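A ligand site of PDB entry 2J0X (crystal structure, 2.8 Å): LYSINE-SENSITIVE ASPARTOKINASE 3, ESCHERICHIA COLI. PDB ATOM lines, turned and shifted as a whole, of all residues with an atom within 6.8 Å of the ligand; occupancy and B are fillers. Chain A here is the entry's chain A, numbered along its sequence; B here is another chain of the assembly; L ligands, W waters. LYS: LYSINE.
An oxygen (O) of the ligand is in hydrogen-bond range of the backbone NH (N) of Phe 324 (2.9 Å). The backbone carbonyl oxygen of Ser 345 is in hydrogen-bond range of a nitrogen (NZ) of the ligand, at 2.8 Å. O of Ser 321 lies within hydrogen-bond range of N of the ligand, at 3.1 Å. A nitrogen (NZ) of the ligand lies within salt-bridge range of the side-chain carboxylate of Asp 340 of chain B, at 3.4 Å. An oxygen (O) of the ligand lies within hydrogen-bond range of the backbone NH (N) of Leu 325 (3.2 Å). O of Val 339 of chain B lies within hydrogen-bond range of N of the ligand (2.6 Å). A nitrogen (N) of the ligand is in hydrogen-bond range of the side-chain hydroxyl of Ser 338 of chain B (2.8 Å). The backbone carbonyl oxygen of Asp 340 of chain B sits at hydrogen-bond distance from a nitrogen (NZ) of the ligand, 3.3 Å away. A nitrogen (NZ) of the ligand is in hydrogen-bond range of the backbone carbonyl oxygen (O) of Glu 346 (2.7 Å). An oxygen (OXT) of the ligand is in hydrogen-bond range of the backbone NH (N) of Val 339 of chain B (2.6 Å). The backbone carbonyl oxygen (O) of Met 318 lies within hydrogen-bond range of a nitrogen (N) of the ligand (3.1 Å).
Water W1 lies within hydrogen-bond range of N of Gly 323 (2.6 Å), OXT of the ligand (2.8 Å) and O of Ile 337 of chain B (2.8 Å).
Merely in contact with the ligand: Gly 323 and Thr 344. Hydrophobic or aromatic side chains that line the ligand: Met 318, Phe 324, Leu 325 and Val 339 of chain B. Within 4 Å of the ligand: Met 318, Ser 321, Gly 323, Phe 324, Leu 325, Thr 344, Ser 345, Glu 346, Ser 338 of chain B, Val 339 of chain B and Asp 340 of chain B. The nearest printed residue that does not touch the ligand is Arg 322 (4.1 Å).
The side-chain hydroxyl (OG) of Ser 321 sits close to the backbone carbonyl oxygen (O) of Asn 317 (3.4 Å). The backbone carbonyl oxygen (O) of Ser 338 of chain B sits at hydrogen-bond distance from the backbone NH (N) of Asp 354 of chain B, at 2.6 Å. The backbone carbonyl oxygen (O) of Ser 321 sits at hydrogen-bond distance from the side-chain hydroxyl (OG) of Ser 338 of chain B (2.7 Å). The backbone NH of Ile 342 of chain B lies within hydrogen-bond range of the side-chain hydroxyl of Thr 344 (2.8 Å). OG of Ser 321 lies within hydrogen-bond range of O of Met 318, 3.4 Å away. The side-chain hydroxyl (OG1) of Thr 344 sits at hydrogen-bond distance from the backbone carbonyl oxygen (O) of Asp 340 of chain B (3.4 Å). OG of Ser 345 lies within hydrogen-bond range of N of Val 347 (3.3 Å). The side-chain sulfur of Met 318 is in hydrogen-bond range of the backbone NH of Ser 348 (3.4 Å).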
ATOM      1  N   ASN A 317      -8.754   4.532   8.253  1.00  0.00           N
ATOM      2  CA  ASN A 317      -7.735   3.700   8.850  1.00  0.00           C
ATOM      3  C   ASN A 317      -6.284   4.005   8.489  1.00  0.00           C
ATOM      4  O   ASN A 317      -5.358   3.467   9.110  1.00  0.00           O
ATOM      5  CB  ASN A 317      -8.042   2.237   8.555  1.00  0.00           C
ATOM      6  CG  ASN A 317      -9.495   1.883   8.846  1.00  0.00           C
ATOM      7  OD1 ASN A 317     -10.035   2.242   9.899  1.00  0.00           O
ATOM      8  ND2 ASN A 317     -10.122   1.163   7.920  1.00  0.00           N
ATOM      9  N   MET A 318      -6.071   4.870   7.487  1.00  0.00           N
ATOM     10  CA  MET A 318      -4.700   5.204   7.133  1.00  0.00           C
ATOM     11  C   MET A 318      -4.144   6.203   8.126  1.00  0.00           C
ATOM     12  O   MET A 318      -2.929   6.312   8.301  1.00  0.00           O
ATOM     13  CB  MET A 318      -4.628   5.741   5.685  1.00  0.00           C
ATOM     14  CG  MET A 318      -5.498   6.930   5.337  1.00  0.00           C
ATOM     15  SD  MET A 318      -5.157   7.508   3.607  1.00  0.00           S
ATOM     16  CE  MET A 318      -6.170   6.347   2.665  1.00  0.00           C
ATOM     17  N   LEU A 319      -5.054   6.882   8.813  1.00  0.00           N
ATOM     18  CA  LEU A 319      -4.697   7.876   9.808  1.00  0.00           C
ATOM     19  C   LEU A 319      -3.835   7.305  10.930  1.00  0.00           C
ATOM     20  O   LEU A 319      -4.307   6.507  11.731  1.00  0.00           O
ATOM     21  CB  LEU A 319      -5.965   8.464  10.428  1.00  0.00           C
ATOM     22  CG  LEU A 319      -6.150   9.991  10.399  1.00  0.00           C
ATOM     23  CD1 LEU A 319      -7.343  10.354  11.256  1.00  0.00           C
ATOM     24  CD2 LEU A 319      -4.915  10.673  10.922  1.00  0.00           C
ATOM     25  N   HIS A 320      -2.572   7.714  10.985  1.00  0.00           N
ATOM     26  CA  HIS A 320      -1.658   7.239  12.033  1.00  0.00           C
ATOM     27  C   HIS A 320      -1.238   5.781  11.878  1.00  0.00           C
ATOM     28  O   HIS A 320      -0.549   5.238  12.749  1.00  0.00           O
ATOM     29  CB  HIS A 320      -2.274   7.413  13.422  1.00  0.00           C
ATOM     30  CG  HIS A 320      -2.917   8.746  13.629  1.00  0.00           C
ATOM     31  ND1 HIS A 320      -2.277   9.931  13.329  1.00  0.00           N
ATOM     32  CD2 HIS A 320      -4.117   9.079  14.138  1.00  0.00           C
ATOM     33  CE1 HIS A 320      -3.068  10.939  13.648  1.00  0.00           C
ATOM     34  NE2 HIS A 320      -4.196  10.451  14.142  1.00  0.00           N
ATOM     35  N   SER A 321      -1.678   5.137  10.800  1.00  0.00           N
ATOM     36  CA  SER A 321      -1.292   3.745  10.587  1.00  0.00           C
ATOM     37  C   SER A 321       0.031   3.663   9.828  1.00  0.00           C
ATOM     38  O   SER A 321       0.387   4.585   9.080  1.00  0.00           O
ATOM     39  CB  SER A 321      -2.364   3.021   9.783  1.00  0.00           C
ATOM     40  OG  SER A 321      -2.023   3.018   8.416  1.00  0.00           O
ATOM     41  N   ARG A 322       0.763   2.572  10.014  1.00  0.00           N
ATOM     42  CA  ARG A 322       2.033   2.375   9.316  1.00  0.00           C
ATOM     43  C   ARG A 322       1.775   1.319   8.258  1.00  0.00           C
ATOM     44  O   ARG A 322       1.011   0.388   8.490  1.00  0.00           O
ATOM     45  CB  ARG A 322       3.129   1.849  10.249  1.00  0.00           C
ATOM     46  CG  ARG A 322       3.410   2.684  11.466  1.00  0.00           C
ATOM     47  CD  ARG A 322       4.123   1.816  12.500  1.00  0.00           C
ATOM     48  NE  ARG A 322       4.011   2.381  13.840  1.00  0.00           N
ATOM     49  CZ  ARG A 322       4.443   1.760  14.934  1.00  0.00           C
ATOM     50  NH1 ARG A 322       4.988   0.559  14.848  1.00  0.00           N
ATOM     51  NH2 ARG A 322       4.316   2.340  16.124  1.00  0.00           N
ATOM     52  N   GLY A 323       2.408   1.477   7.104  1.00  0.00           N
ATOM     53  CA  GLY A 323       2.260   0.491   6.050  1.00  0.00           C
ATOM     54  C   GLY A 323       0.986   0.451   5.221  1.00  0.00           C
ATOM     55  O   GLY A 323       0.846  -0.452   4.405  1.00  0.00           O
ATOM     56  N   PHE A 324       0.068   1.398   5.395  1.00  0.00           N
ATOM     57  CA  PHE A 324      -1.149   1.367   4.582  1.00  0.00           C
ATOM     58  C   PHE A 324      -0.746   1.530   3.142  1.00  0.00           C
ATOM     59  O   PHE A 324      -1.196   0.784   2.273  1.00  0.00           O
ATOM     60  CB  PHE A 324      -2.106   2.512   4.930  1.00  0.00           C
ATOM     61  CG  PHE A 324      -3.396   2.509   4.111  1.00  0.00           C
ATOM     62  CD1 PHE A 324      -4.547   1.918   4.606  1.00  0.00           C
ATOM     63  CD2 PHE A 324      -3.436   3.104   2.854  1.00  0.00           C
ATOM     64  CE1 PHE A 324      -5.743   1.924   3.857  1.00  0.00           C
ATOM     65  CE2 PHE A 324      -4.619   3.106   2.104  1.00  0.00           C
ATOM     66  CZ  PHE A 324      -5.774   2.523   2.603  1.00  0.00           C
ATOM     67  N   LEU A 325       0.090   2.520   2.876  1.00  0.00           N
ATOM     68  CA  LEU A 325       0.530   2.763   1.506  1.00  0.00           C
ATOM     69  C   LEU A 325       1.474   1.670   1.058  1.00  0.00           C
ATOM     70  O   LEU A 325       1.461   1.273  -0.093  1.00  0.00           O
ATOM     71  CB  LEU A 325       1.196   4.133   1.395  1.00  0.00           C
ATOM     72  CG  LEU A 325       0.269   5.331   1.613  1.00  0.00           C
ATOM     73  CD1 LEU A 325       1.118   6.595   1.701  1.00  0.00           C
ATOM     74  CD2 LEU A 325      -0.742   5.445   0.480  1.00  0.00           C
ATOM     75  N   ALA A 326       2.295   1.178   1.983  1.00  0.00           N
ATOM     76  CA  ALA A 326       3.234   0.127   1.634  1.00  0.00           C
ATOM     77  C   ALA A 326       2.449  -1.002   0.980  1.00  0.00           C
ATOM     78  O   ALA A 326       2.895  -1.590  -0.009  1.00  0.00           O
ATOM     79  CB  ALA A 326       3.937  -0.375   2.886  1.00  0.00           C
ATOM     80  N   GLU A 327       1.277  -1.276   1.525  1.00  0.00           N
ATOM     81  CA  GLU A 327       0.440  -2.357   1.003  1.00  0.00           C
ATOM     82  C   GLU A 327      -0.291  -1.987  -0.268  1.00  0.00           C
ATOM     83  O   GLU A 327      -0.392  -2.778  -1.197  1.00  0.00           O
ATOM     84  CB  GLU A 327      -0.593  -2.813   2.055  1.00  0.00           C
ATOM     85  CG  GLU A 327      -1.474  -3.952   1.549  1.00  0.00           C
ATOM     86  CD  GLU A 327      -2.382  -4.545   2.624  1.00  0.00           C
ATOM     87  OE1 GLU A 327      -3.114  -5.513   2.291  1.00  0.00           O
ATOM     88  OE2 GLU A 327      -2.371  -4.073   3.776  1.00  0.00           O
ATOM     89  N   THR A 343      -0.937  12.628  -4.361  1.00  0.00           N
ATOM     90  CA  THR A 343      -1.270  13.751  -3.484  1.00  0.00           C
ATOM     91  C   THR A 343      -2.000  13.143  -2.305  1.00  0.00           C
ATOM     92  O   THR A 343      -2.700  12.130  -2.445  1.00  0.00           O
ATOM     93  CB  THR A 343      -2.212  14.749  -4.164  1.00  0.00           C
ATOM     94  OG1 THR A 343      -2.473  15.839  -3.273  1.00  0.00           O
ATOM     95  CG2 THR A 343      -3.535  14.085  -4.494  1.00  0.00           C
ATOM     96  N   THR A 344      -1.862  13.747  -1.131  1.00  0.00           N
ATOM     97  CA  THR A 344      -2.509  13.201   0.041  1.00  0.00           C
ATOM     98  C   THR A 344      -3.260  14.206   0.885  1.00  0.00           C
ATOM     99  O   THR A 344      -2.989  15.411   0.844  1.00  0.00           O
ATOM    100  CB  THR A 344      -1.472  12.499   0.957  1.00  0.00           C
ATOM    101  OG1 THR A 344      -0.486  13.456   1.370  1.00  0.00           O
ATOM    102  CG2 THR A 344      -0.808  11.337   0.213  1.00  0.00           C
ATOM    103  N   SER A 345      -4.213  13.690   1.654  1.00  0.00           N
ATOM    104  CA  SER A 345      -4.999  14.482   2.569  1.00  0.00           C
ATOM    105  C   SER A 345      -4.826  13.685   3.857  1.00  0.00           C
ATOM    106  O   SER A 345      -4.043  12.749   3.888  1.00  0.00           O
ATOM    107  CB  SER A 345      -6.481  14.529   2.165  1.00  0.00           C
ATOM    108  OG  SER A 345      -7.268  13.631   2.912  1.00  0.00           O
ATOM    109  N   GLU A 346      -5.538  14.052   4.912  1.00  0.00           N
ATOM    110  CA  GLU A 346      -5.381  13.327   6.149  1.00  0.00           C
ATOM    111  C   GLU A 346      -5.805  11.869   6.046  1.00  0.00           C
ATOM    112  O   GLU A 346      -5.044  10.973   6.403  1.00  0.00           O
ATOM    113  CB  GLU A 346      -6.167  14.026   7.268  1.00  0.00           C
ATOM    114  CG  GLU A 346      -5.519  15.294   7.776  1.00  0.00           C
ATOM    115  CD  GLU A 346      -4.102  15.070   8.270  1.00  0.00           C
ATOM    116  OE1 GLU A 346      -3.233  14.699   7.454  1.00  0.00           O
ATOM    117  OE2 GLU A 346      -3.866  15.257   9.484  1.00  0.00           O
ATOM    118  N   VAL A 347      -7.025  11.625   5.550  1.00  0.00           N
ATOM    119  CA  VAL A 347      -7.535  10.260   5.447  1.00  0.00           C
ATOM    120  C   VAL A 347      -7.818   9.796   4.029  1.00  0.00           C
ATOM    121  O   VAL A 347      -8.691   8.950   3.816  1.00  0.00           O
ATOM    122  CB  VAL A 347      -8.847  10.056   6.247  1.00  0.00           C
ATOM    123  CG1 VAL A 347      -8.618  10.338   7.730  1.00  0.00           C
ATOM    124  CG2 VAL A 347      -9.955  10.927   5.675  1.00  0.00           C
ATOM    125  N   SER A 348      -7.067  10.327   3.069  1.00  0.00           N
ATOM    126  CA  SER A 348      -7.290   9.953   1.683  1.00  0.00           C
ATOM    127  C   SER A 348      -6.056  10.246   0.834  1.00  0.00           C
ATOM    128  O   SER A 348      -5.336  11.199   1.094  1.00  0.00           O
ATOM    129  CB  SER A 348      -8.489  10.754   1.148  1.00  0.00           C
ATOM    130  OG  SER A 348      -8.786  10.414  -0.190  1.00  0.00           O
ATOM    131  N   VAL A 349      -5.834   9.408  -0.175  1.00  0.00           N
ATOM    132  CA  VAL A 349      -4.715   9.570  -1.081  1.00  0.00           C
ATOM    133  C   VAL A 349      -5.192   9.424  -2.523  1.00  0.00           C
ATOM    134  O   VAL A 349      -5.965   8.526  -2.840  1.00  0.00           O
ATOM    135  CB  VAL A 349      -3.620   8.505  -0.846  1.00  0.00           C
ATOM    136  CG1 VAL A 349      -4.217   7.122  -0.999  1.00  0.00           C
ATOM    137  CG2 VAL A 349      -2.507   8.698  -1.854  1.00  0.00           C
ATOM    138  N   PHE B 329       8.008   2.583   0.796  1.00  0.00           N
ATOM    139  CA  PHE B 329       7.005   2.554   1.845  1.00  0.00           C
ATOM    140  C   PHE B 329       7.151   1.294   2.675  1.00  0.00           C
ATOM    141  O   PHE B 329       6.817   1.278   3.861  1.00  0.00           O
ATOM    142  CB  PHE B 329       5.589   2.627   1.239  1.00  0.00           C
ATOM    143  CG  PHE B 329       5.235   3.989   0.698  1.00  0.00           C
ATOM    144  CD1 PHE B 329       4.857   4.160  -0.627  1.00  0.00           C
ATOM    145  CD2 PHE B 329       5.333   5.123   1.517  1.00  0.00           C
ATOM    146  CE1 PHE B 329       4.586   5.431  -1.131  1.00  0.00           C
ATOM    147  CE2 PHE B 329       5.062   6.394   1.013  1.00  0.00           C
ATOM    148  CZ  PHE B 329       4.690   6.544  -0.313  1.00  0.00           C
ATOM    149  N   ILE B 337       7.369   3.834  10.843  1.00  0.00           N
ATOM    150  CA  ILE B 337       7.115   5.219  10.466  1.00  0.00           C
ATOM    151  C   ILE B 337       5.814   5.313   9.711  1.00  0.00           C
ATOM    152  O   ILE B 337       5.531   4.505   8.838  1.00  0.00           O
ATOM    153  CB  ILE B 337       8.211   5.752   9.537  1.00  0.00           C
ATOM    154  CG1 ILE B 337       9.533   5.840  10.284  1.00  0.00           C
ATOM    155  CG2 ILE B 337       7.813   7.118   8.992  1.00  0.00           C
ATOM    156  CD1 ILE B 337      10.695   6.178   9.379  1.00  0.00           C
ATOM    157  N   SER B 338       5.006   6.310  10.056  1.00  0.00           N
ATOM    158  CA  SER B 338       3.749   6.506   9.363  1.00  0.00           C
ATOM    159  C   SER B 338       3.955   7.741   8.509  1.00  0.00           C
ATOM    160  O   SER B 338       4.441   8.766   8.975  1.00  0.00           O
ATOM    161  CB  SER B 338       2.620   6.720  10.360  1.00  0.00           C
ATOM    162  OG  SER B 338       1.405   7.006   9.685  1.00  0.00           O
ATOM    163  N   VAL B 339       3.612   7.610   7.230  1.00  0.00           N
ATOM    164  CA  VAL B 339       3.752   8.713   6.278  1.00  0.00           C
ATOM    165  C   VAL B 339       2.467   9.533   6.287  1.00  0.00           C
ATOM    166  O   VAL B 339       1.373   8.977   6.269  1.00  0.00           O
ATOM    167  CB  VAL B 339       4.005   8.167   4.840  1.00  0.00           C
ATOM    168  CG1 VAL B 339       4.155   9.308   3.854  1.00  0.00           C
ATOM    169  CG2 VAL B 339       5.269   7.298   4.808  1.00  0.00           C
ATOM    170  N   ASP B 340       2.599  10.865   6.358  1.00  0.00           N
ATOM    171  CA  ASP B 340       1.414  11.716   6.342  1.00  0.00           C
ATOM    172  C   ASP B 340       1.229  12.300   4.947  1.00  0.00           C
ATOM    173  O   ASP B 340       0.493  11.747   4.138  1.00  0.00           O
ATOM    174  CB  ASP B 340       1.506  12.845   7.362  1.00  0.00           C
ATOM    175  CG  ASP B 340       0.298  13.789   7.296  1.00  0.00           C
ATOM    176  OD1 ASP B 340      -0.828  13.324   6.982  1.00  0.00           O
ATOM    177  OD2 ASP B 340       0.471  14.994   7.579  1.00  0.00           O
ATOM    178  N   LEU B 341       1.920  13.399   4.646  1.00  0.00           N
ATOM    179  CA  LEU B 341       1.806  14.032   3.342  1.00  0.00           C
ATOM    180  C   LEU B 341       2.771  13.448   2.303  1.00  0.00           C
ATOM    181  O   LEU B 341       3.887  13.048   2.621  1.00  0.00           O
ATOM    182  CB  LEU B 341       2.030  15.541   3.460  1.00  0.00           C
ATOM    183  CG  LEU B 341       1.195  16.335   4.478  1.00  0.00           C
ATOM    184  CD1 LEU B 341       1.455  17.817   4.281  1.00  0.00           C
ATOM    185  CD2 LEU B 341      -0.294  16.045   4.297  1.00  0.00           C
ATOM    186  N   ILE B 342       2.312  13.404   1.052  1.00  0.00           N
ATOM    187  CA  ILE B 342       3.120  12.901  -0.054  1.00  0.00           C
ATOM    188  C   ILE B 342       2.865  13.712  -1.310  1.00  0.00           C
ATOM    189  O   ILE B 342       1.728  13.927  -1.681  1.00  0.00           O
ATOM    190  CB  ILE B 342       2.773  11.456  -0.439  1.00  0.00           C
ATOM    191  CG1 ILE B 342       2.797  10.559   0.795  1.00  0.00           C
ATOM    192  CG2 ILE B 342       3.777  10.956  -1.478  1.00  0.00           C
ATOM    193  CD1 ILE B 342       2.473   9.119   0.466  1.00  0.00           C
ATOM    194  N   ASP B 354       4.493  11.193   9.836  1.00  0.00           N
ATOM    195  CA  ASP B 354       3.310  11.262  10.680  1.00  0.00           C
ATOM    196  C   ASP B 354       3.825  11.049  12.095  1.00  0.00           C
ATOM    197  O   ASP B 354       4.044   9.906  12.507  1.00  0.00           O
ATOM    198  CB  ASP B 354       2.359  10.133  10.267  1.00  0.00           C
ATOM    199  CG  ASP B 354       1.141  10.013  11.162  1.00  0.00           C
ATOM    200  OD1 ASP B 354       1.211  10.415  12.336  1.00  0.00           O
ATOM    201  OD2 ASP B 354       0.104   9.506  10.676  1.00  0.00           O
HETATM  202  N   LYS L   1      -0.146   7.076   7.313  1.00  0.00           N
HETATM  203  CA  LYS L   1      -0.381   6.133   6.213  1.00  0.00           C
HETATM  204  C   LYS L   1       0.869   5.332   5.921  1.00  0.00           C
HETATM  205  O   LYS L   1       0.833   4.195   5.449  1.00  0.00           O
HETATM  206  CB  LYS L   1      -0.818   6.863   4.948  1.00  0.00           C
HETATM  207  CG  LYS L   1      -1.781   8.011   5.067  1.00  0.00           C
HETATM  208  CD  LYS L   1      -1.571   9.034   3.964  1.00  0.00           C
HETATM  209  CE  LYS L   1      -2.516  10.223   4.028  1.00  0.00           C
HETATM  210  NZ  LYS L   1      -2.526  10.928   5.332  1.00  0.00           N
HETATM  211  OXT LYS L   1       2.034   5.897   6.162  1.00  0.00           O
HETATM  212  O   HOH W   1       3.603   3.745   6.885  1.00  0.00           O
